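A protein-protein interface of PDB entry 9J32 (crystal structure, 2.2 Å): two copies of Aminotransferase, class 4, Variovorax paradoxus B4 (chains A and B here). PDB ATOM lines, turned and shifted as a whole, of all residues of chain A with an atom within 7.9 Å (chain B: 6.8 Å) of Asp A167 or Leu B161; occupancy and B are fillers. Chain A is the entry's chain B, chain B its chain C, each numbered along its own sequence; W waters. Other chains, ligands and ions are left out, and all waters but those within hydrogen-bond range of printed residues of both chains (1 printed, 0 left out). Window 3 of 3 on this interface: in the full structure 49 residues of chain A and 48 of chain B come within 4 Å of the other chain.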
ATOM      1  N   SER A  80      22.840   8.988  -5.021  1.00  0.00           N
ATOM      2  CA  SER A  80      21.876   8.328  -5.884  1.00  0.00           C
ATOM      3  C   SER A  80      21.713   9.047  -7.249  1.00  0.00           C
ATOM      4  O   SER A  80      21.443   8.373  -8.251  1.00  0.00           O
ATOM      5  CB  SER A  80      20.551   8.171  -5.149  1.00  0.00           C
ATOM      6  OG  SER A  80      19.862   9.398  -5.146  1.00  0.00           O
ATOM      7  N   SER A 164       5.055   7.457  -6.197  1.00  0.00           N
ATOM      8  CA  SER A 164       5.643   6.664  -7.265  1.00  0.00           C
ATOM      9  C   SER A 164       6.423   5.522  -6.682  1.00  0.00           C
ATOM     10  O   SER A 164       7.007   5.644  -5.608  1.00  0.00           O
ATOM     11  CB  SER A 164       6.598   7.501  -8.125  1.00  0.00           C
ATOM     12  OG  SER A 164       7.301   8.495  -7.377  1.00  0.00           O
ATOM     13  N   GLY A 165       6.567   4.475  -7.496  1.00  0.00           N
ATOM     14  CA  GLY A 165       7.584   3.485  -7.246  1.00  0.00           C
ATOM     15  C   GLY A 165       8.980   3.962  -7.635  1.00  0.00           C
ATOM     16  O   GLY A 165       9.104   4.885  -8.404  1.00  0.00           O
ATOM     17  N   PRO A 166      10.059   3.281  -7.150  1.00  0.00           N
ATOM     18  CA  PRO A 166      11.434   3.690  -7.372  1.00  0.00           C
ATOM     19  C   PRO A 166      11.953   3.618  -8.789  1.00  0.00           C
ATOM     20  O   PRO A 166      12.933   4.292  -9.104  1.00  0.00           O
ATOM     21  CB  PRO A 166      12.283   2.751  -6.476  1.00  0.00           C
ATOM     22  CG  PRO A 166      11.377   1.552  -6.345  1.00  0.00           C
ATOM     23  CD  PRO A 166       9.998   2.160  -6.181  1.00  0.00           C
ATOM     24  N   ASP A 167      11.373   2.783  -9.614  1.00  0.00           N
ATOM     25  CA  ASP A 167      11.616   2.858 -11.053  1.00  0.00           C
ATOM     26  C   ASP A 167      10.993   4.055 -11.792  1.00  0.00           C
ATOM     27  O   ASP A 167      11.182   4.155 -13.027  1.00  0.00           O
ATOM     28  CB  ASP A 167      11.071   1.613 -11.737  1.00  0.00           C
ATOM     29  CG  ASP A 167       9.591   1.393 -11.642  1.00  0.00           C
ATOM     30  OD1 ASP A 167       8.980   2.000 -10.720  1.00  0.00           O
ATOM     31  OD2 ASP A 167       9.093   0.607 -12.459  1.00  0.00           O
ATOM     32  N   VAL A 168      10.119   4.837 -11.126  1.00  0.00           N
ATOM     33  CA  VAL A 168       9.590   6.076 -11.694  1.00  0.00           C
ATOM     34  C   VAL A 168      10.340   7.244 -11.069  1.00  0.00           C
ATOM     35  O   VAL A 168      10.961   8.042 -11.779  1.00  0.00           O
ATOM     36  CB  VAL A 168       8.070   6.163 -11.468  1.00  0.00           C
ATOM     37  CG1 VAL A 168       7.505   7.549 -11.719  1.00  0.00           C
ATOM     38  CG2 VAL A 168       7.368   5.100 -12.299  1.00  0.00           C
ATOM     39  N   PHE A 169      10.313   7.306  -9.734  1.00  0.00           N
ATOM     40  CA  PHE A 169      10.993   8.352  -8.982  1.00  0.00           C
ATOM     41  C   PHE A 169      10.903   7.957  -7.508  1.00  0.00           C
ATOM     42  O   PHE A 169       9.782   7.856  -6.969  1.00  0.00           O
ATOM     43  CB  PHE A 169      10.314   9.718  -9.180  1.00  0.00           C
ATOM     44  CG  PHE A 169      11.022  10.942  -8.613  1.00  0.00           C
ATOM     45  CD1 PHE A 169      10.937  11.246  -7.262  1.00  0.00           C
ATOM     46  CD2 PHE A 169      11.765  11.761  -9.418  1.00  0.00           C
ATOM     47  CE1 PHE A 169      11.540  12.387  -6.750  1.00  0.00           C
ATOM     48  CE2 PHE A 169      12.340  12.912  -8.930  1.00  0.00           C
ATOM     49  CZ  PHE A 169      12.250  13.226  -7.593  1.00  0.00           C
ATOM     50  N   ASP A 170      12.070   7.666  -6.947  1.00  0.00           N
ATOM     51  CA  ASP A 170      12.235   7.217  -5.578  1.00  0.00           C
ATOM     52  C   ASP A 170      11.965   8.382  -4.622  1.00  0.00           C
ATOM     53  O   ASP A 170      12.758   9.335  -4.547  1.00  0.00           O
ATOM     54  CB  ASP A 170      13.649   6.731  -5.334  1.00  0.00           C
ATOM     55  CG  ASP A 170      13.862   6.036  -3.981  1.00  0.00           C
ATOM     56  OD1 ASP A 170      12.929   6.018  -3.158  1.00  0.00           O
ATOM     57  OD2 ASP A 170      14.922   5.384  -3.816  1.00  0.00           O
ATOM     58  N   PRO A 201       1.397   3.042  -5.003  1.00  0.00           N
ATOM     59  CA  PRO A 201       0.864   2.518  -6.245  1.00  0.00           C
ATOM     60  C   PRO A 201      -0.091   1.358  -6.046  1.00  0.00           C
ATOM     61  O   PRO A 201      -0.867   1.111  -6.948  1.00  0.00           O
ATOM     62  CB  PRO A 201       2.067   2.219  -7.137  1.00  0.00           C
ATOM     63  CG  PRO A 201       3.232   2.810  -6.431  1.00  0.00           C
ATOM     64  CD  PRO A 201       2.868   2.902  -4.986  1.00  0.00           C
ATOM     65  N   TYR A 228       7.419   3.379  -0.345  1.00  0.00           N
ATOM     66  CA  TYR A 228       6.946   4.319  -1.369  1.00  0.00           C
ATOM     67  C   TYR A 228       6.797   5.754  -0.818  1.00  0.00           C
ATOM     68  O   TYR A 228       6.056   6.542  -1.389  1.00  0.00           O
ATOM     69  CB  TYR A 228       5.618   3.784  -1.877  1.00  0.00           C
ATOM     70  CG  TYR A 228       5.565   2.420  -2.562  1.00  0.00           C
ATOM     71  CD1 TYR A 228       6.168   2.215  -3.804  1.00  0.00           C
ATOM     72  CD2 TYR A 228       4.845   1.368  -2.055  1.00  0.00           C
ATOM     73  CE1 TYR A 228       6.176   0.983  -4.431  1.00  0.00           C
ATOM     74  CE2 TYR A 228       4.778   0.126  -2.704  1.00  0.00           C
ATOM     75  CZ  TYR A 228       5.400  -0.052  -3.914  1.00  0.00           C
ATOM     76  OH  TYR A 228       5.364  -1.205  -4.629  1.00  0.00           O
ATOM     77  N   THR B 158      17.997   2.288 -23.564  1.00  0.00           N
ATOM     78  CA  THR B 158      16.687   2.242 -22.888  1.00  0.00           C
ATOM     79  C   THR B 158      16.905   2.066 -21.372  1.00  0.00           C
ATOM     80  O   THR B 158      17.173   0.961 -20.907  1.00  0.00           O
ATOM     81  CB  THR B 158      15.773   1.156 -23.458  1.00  0.00           C
ATOM     82  OG1 THR B 158      15.769   1.293 -24.867  1.00  0.00           O
ATOM     83  CG2 THR B 158      14.315   1.328 -23.064  1.00  0.00           C
ATOM     84  N   SER B 159      16.791   3.186 -20.629  1.00  0.00           N
ATOM     85  CA  SER B 159      16.816   3.190 -19.195  1.00  0.00           C
ATOM     86  C   SER B 159      15.778   2.228 -18.578  1.00  0.00           C
ATOM     87  O   SER B 159      14.684   1.966 -19.102  1.00  0.00           O
ATOM     88  CB  SER B 159      16.613   4.608 -18.622  1.00  0.00           C
ATOM     89  OG  SER B 159      16.735   4.587 -17.191  1.00  0.00           O
ATOM     90  N   THR B 160      16.143   1.786 -17.369  1.00  0.00           N
ATOM     91  CA  THR B 160      15.288   1.007 -16.526  1.00  0.00           C
ATOM     92  C   THR B 160      14.215   1.887 -15.906  1.00  0.00           C
ATOM     93  O   THR B 160      13.214   1.312 -15.447  1.00  0.00           O
ATOM     94  CB  THR B 160      16.121   0.260 -15.500  1.00  0.00           C
ATOM     95  OG1 THR B 160      15.327  -0.834 -15.021  1.00  0.00           O
ATOM     96  CG2 THR B 160      16.495   1.129 -14.312  1.00  0.00           C
ATOM     97  N   LEU B 161      14.429   3.219 -15.876  1.00  0.00           N
ATOM     98  CA  LEU B 161      13.514   4.190 -15.287  1.00  0.00           C
ATOM     99  C   LEU B 161      12.432   4.560 -16.289  1.00  0.00           C
ATOM    100  O   LEU B 161      12.677   4.774 -17.468  1.00  0.00           O
ATOM    101  CB  LEU B 161      14.198   5.415 -14.676  1.00  0.00           C
ATOM    102  CG  LEU B 161      15.355   5.051 -13.723  1.00  0.00           C
ATOM    103  CD1 LEU B 161      16.289   6.230 -13.314  1.00  0.00           C
ATOM    104  CD2 LEU B 161      14.824   4.335 -12.477  1.00  0.00           C
ATOM    105  N   ARG B 162      11.198   4.641 -15.772  1.00  0.00           N
ATOM    106  CA  ARG B 162       9.982   4.612 -16.538  1.00  0.00           C
ATOM    107  C   ARG B 162       9.378   5.995 -16.504  1.00  0.00           C
ATOM    108  O   ARG B 162       9.458   6.652 -15.484  1.00  0.00           O
ATOM    109  CB  ARG B 162       8.980   3.635 -15.931  1.00  0.00           C
ATOM    110  CG  ARG B 162       9.322   2.157 -16.019  1.00  0.00           C
ATOM    111  CD  ARG B 162       9.137   1.732 -17.430  1.00  0.00           C
ATOM    112  NE  ARG B 162       9.267   0.276 -17.407  1.00  0.00           N
ATOM    113  CZ  ARG B 162      10.334  -0.430 -17.732  1.00  0.00           C
ATOM    114  NH1 ARG B 162      11.392   0.165 -18.219  1.00  0.00           N
ATOM    115  NH2 ARG B 162      10.318  -1.746 -17.651  1.00  0.00           N
ATOM    116  N   CYS B 163       8.694   6.325 -17.609  1.00  0.00           N
ATOM    117  CA  CYS B 163       7.734   7.390 -17.643  1.00  0.00           C
ATOM    118  C   CYS B 163       6.644   7.100 -16.610  1.00  0.00           C
ATOM    119  O   CYS B 163       6.233   5.927 -16.485  1.00  0.00           O
ATOM    120  CB  CYS B 163       7.070   7.474 -19.026  1.00  0.00           C
ATOM    121  SG  CYS B 163       8.232   7.925 -20.345  1.00  0.00           S
ATOM    122  N   LEU B 179      14.321  15.844 -12.200  1.00  0.00           N
ATOM    123  CA  LEU B 179      15.159  14.765 -11.748  1.00  0.00           C
ATOM    124  C   LEU B 179      14.641  13.429 -12.280  1.00  0.00           C
ATOM    125  O   LEU B 179      15.435  12.497 -12.439  1.00  0.00           O
ATOM    126  CB  LEU B 179      15.335  14.777 -10.227  1.00  0.00           C
ATOM    127  CG  LEU B 179      16.543  15.571  -9.723  1.00  0.00           C
ATOM    128  CD1 LEU B 179      16.464  15.674  -8.241  1.00  0.00           C
ATOM    129  CD2 LEU B 179      17.851  14.947 -10.136  1.00  0.00           C
ATOM    130  N   ASN B 180      13.331  13.354 -12.589  1.00  0.00           N
ATOM    131  CA  ASN B 180      12.733  12.143 -13.152  1.00  0.00           C
ATOM    132  C   ASN B 180      13.394  11.764 -14.498  1.00  0.00           C
ATOM    133  O   ASN B 180      13.753  10.610 -14.754  1.00  0.00           O
ATOM    134  CB  ASN B 180      11.207  12.274 -13.133  1.00  0.00           C
ATOM    135  CG  ASN B 180      10.665  13.374 -14.039  1.00  0.00           C
ATOM    136  OD1 ASN B 180      11.377  14.279 -14.446  1.00  0.00           O
ATOM    137  ND2 ASN B 180       9.388  13.424 -14.303  1.00  0.00           N
ATOM    138  N   LEU B 181      13.626  12.766 -15.335  1.00  0.00           N
ATOM    139  CA  LEU B 181      14.248  12.590 -16.624  1.00  0.00           C
ATOM    140  C   LEU B 181      15.751  12.491 -16.490  1.00  0.00           C
ATOM    141  O   LEU B 181      16.356  11.695 -17.208  1.00  0.00           O
ATOM    142  CB  LEU B 181      13.849  13.726 -17.553  1.00  0.00           C
ATOM    143  CG  LEU B 181      12.335  13.940 -17.731  1.00  0.00           C
ATOM    144  CD1 LEU B 181      12.012  15.274 -18.412  1.00  0.00           C
ATOM    145  CD2 LEU B 181      11.746  12.794 -18.493  1.00  0.00           C
ATOM    146  N   ILE B 182      16.352  13.321 -15.629  1.00  0.00           N
ATOM    147  CA  ILE B 182      17.801  13.345 -15.430  1.00  0.00           C
ATOM    148  C   ILE B 182      18.291  11.971 -14.978  1.00  0.00           C
ATOM    149  O   ILE B 182      19.365  11.539 -15.365  1.00  0.00           O
ATOM    150  CB  ILE B 182      18.240  14.447 -14.423  1.00  0.00           C
ATOM    151  CG1 ILE B 182      18.070  15.829 -14.997  1.00  0.00           C
ATOM    152  CG2 ILE B 182      19.695  14.280 -13.989  1.00  0.00           C
ATOM    153  CD1 ILE B 182      18.167  16.929 -13.957  1.00  0.00           C
ATOM    154  N   GLN B 183      17.550  11.309 -14.116  1.00  0.00           N
ATOM    155  CA  GLN B 183      17.989  10.000 -13.615  1.00  0.00           C
ATOM    156  C   GLN B 183      18.005   8.964 -14.735  1.00  0.00           C
ATOM    157  O   GLN B 183      18.870   8.132 -14.781  1.00  0.00           O
ATOM    158  CB  GLN B 183      17.213   9.497 -12.403  1.00  0.00           C
ATOM    159  CG  GLN B 183      17.530  10.281 -11.129  1.00  0.00           C
ATOM    160  CD  GLN B 183      16.600   9.936  -9.964  1.00  0.00           C
ATOM    161  OE1 GLN B 183      17.048   9.460  -8.911  1.00  0.00           O
ATOM    162  NE2 GLN B 183      15.291  10.147 -10.117  1.00  0.00           N
ATOM    163  N   ALA B 184      17.044   9.003 -15.646  1.00  0.00           N
ATOM    164  CA  ALA B 184      17.059   8.144 -16.826  1.00  0.00           C
ATOM    165  C   ALA B 184      18.309   8.418 -17.677  1.00  0.00           C
ATOM    166  O   ALA B 184      18.916   7.458 -18.159  1.00  0.00           O
ATOM    167  CB  ALA B 184      15.821   8.384 -17.638  1.00  0.00           C
ATOM    168  N   LEU B 185      18.686   9.711 -17.817  1.00  0.00           N
ATOM    169  CA  LEU B 185      19.874  10.108 -18.566  1.00  0.00           C
ATOM    170  C   LEU B 185      21.152   9.584 -17.926  1.00  0.00           C
ATOM    171  O   LEU B 185      22.013   9.043 -18.617  1.00  0.00           O
ATOM    172  CB  LEU B 185      19.928  11.625 -18.743  1.00  0.00           C
ATOM    173  CG  LEU B 185      21.091  12.141 -19.594  1.00  0.00           C
ATOM    174  CD1 LEU B 185      21.132  11.579 -20.980  1.00  0.00           C
ATOM    175  CD2 LEU B 185      21.065  13.645 -19.682  1.00  0.00           C
ATOM    176  N   GLN B 187      21.690   6.941 -16.143  1.00  0.00           N
ATOM    177  CA  GLN B 187      21.891   5.546 -16.480  1.00  0.00           C
ATOM    178  C   GLN B 187      22.313   5.355 -17.942  1.00  0.00           C
ATOM    179  O   GLN B 187      23.161   4.524 -18.208  1.00  0.00           O
ATOM    180  CB  GLN B 187      20.653   4.691 -16.182  1.00  0.00           C
ATOM    181  CG  GLN B 187      20.968   3.204 -16.282  1.00  0.00           C
ATOM    182  CD  GLN B 187      19.776   2.273 -16.240  1.00  0.00           C
ATOM    183  OE1 GLN B 187      18.671   2.646 -16.646  1.00  0.00           O
ATOM    184  NE2 GLN B 187      20.035   1.031 -15.808  1.00  0.00           N
ATOM    185  N   LEU B 197      16.272   6.420 -23.927  1.00  0.00           N
ATOM    186  CA  LEU B 197      14.941   6.001 -24.316  1.00  0.00           C
ATOM    187  C   LEU B 197      14.245   5.500 -23.046  1.00  0.00           C
ATOM    188  O   LEU B 197      14.873   4.944 -22.172  1.00  0.00           O
ATOM    189  CB  LEU B 197      15.030   4.943 -25.409  1.00  0.00           C
ATOM    190  CG  LEU B 197      13.744   4.582 -26.143  1.00  0.00           C
ATOM    191  CD1 LEU B 197      13.182   5.789 -26.799  1.00  0.00           C
ATOM    192  CD2 LEU B 197      13.956   3.477 -27.186  1.00  0.00           C
ATOM    193  N   MET B 198      12.970   5.811 -22.904  1.00  0.00           N
ATOM    194  CA  MET B 198      12.178   5.428 -21.742  1.00  0.00           C
ATOM    195  C   MET B 198      10.977   4.641 -22.223  1.00  0.00           C
ATOM    196  O   MET B 198      10.345   4.997 -23.243  1.00  0.00           O
ATOM    197  CB  MET B 198      11.735   6.668 -20.937  1.00  0.00           C
ATOM    198  CG  MET B 198      12.943   7.444 -20.401  1.00  0.00           C
ATOM    199  SD  MET B 198      12.508   9.018 -19.653  1.00  0.00           S
ATOM    200  CE  MET B 198      11.971   8.466 -18.042  1.00  0.00           C
ATOM    201  N   LEU B 199      10.603   3.642 -21.398  1.00  0.00           N
ATOM    202  CA  LEU B 199       9.340   2.945 -21.601  1.00  0.00           C
ATOM    203  C   LEU B 199       8.253   3.581 -20.747  1.00  0.00           C
ATOM    204  O   LEU B 199       8.577   4.136 -19.694  1.00  0.00           O
ATOM    205  CB  LEU B 199       9.533   1.483 -21.288  1.00  0.00           C
ATOM    206  CG  LEU B 199      10.684   0.774 -22.032  1.00  0.00           C
ATOM    207  CD1 LEU B 199      10.564  -0.674 -21.736  1.00  0.00           C
ATOM    208  CD2 LEU B 199      10.645   1.025 -23.527  1.00  0.00           C
HETATM  209  O   HOH W   1      13.636   8.867 -11.875  1.00  0.00           O
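O of Asp A167 is in hydrogen-bond range of N of Arg B162 (2.8 Å).
OG of Ser A164 is in hydrogen-bond range of O of Phe A169 (2.6 Å). The side-chain hydroxyl (OG) of Ser B159 is in hydrogen-bond range of the backbone NH (N) of Leu B161 (3.0 Å). The backbone carbonyl oxygen of Leu B179 is in hydrogen-bond range of the side-chain amide nitrogen of Gln B183 (3.3 Å).
Among the printed residues, pairs that only touch across the chains: Pro A166 with Leu B161 (3.9 Å), Asp A167 with Leu B161 (3.2 Å), Val A168 with Arg B162 (3.8 Å), Phe A169 with Leu B179 (3.8 Å), Phe A169 with Asn B180 (3.8 Å) and Phe A169 with Gln B183 (3.9 Å).
Of chain B, only Leu B161 (3.2 Å) and Arg B162 (2.8 Å) come within 4 Å of Asp A167. Of the printed residues of chain B, Val A168 touches Arg B162. Printed residues of chain B within 4 Å of Phe A169: Leu B179 (3.8 Å), Asn B180 (3.8 Å) and Gln B183 (3.9 Å). Leu B161 touches just these residues of chain A: Pro A166 (3.9 Å) and Asp A167 (3.2 Å). Of the printed residues of chain A, Leu B179 touches Phe A169 (3.8 Å). Of the printed residues of chain A, Asn B180 touches Phe A169 (3.8 Å). Of the printed residues of chain A, Gln B183 touches Phe A169. The nearest residue of chain A that does not touch Leu B161 is Val A168 (4.9 Å).
Hydrophobic or aromatic side chains of chain B that line the printed part of chain A: Leu B161 and Leu B179. Among the printed residues, 7 pairs touch across the chains. Among the printed residues, no Asp or Glu carboxylate lies within 4 Å of a Lys or Arg side-chain nitrogen of the other chain.
No position is printed for both chains.
Water W1 lies within hydrogen-bond range of the side-chain amide nitrogen of Gln B183, the backbone carbonyl oxygen of Val A168 and the backbone carbonyl oxygen of Asn B180.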
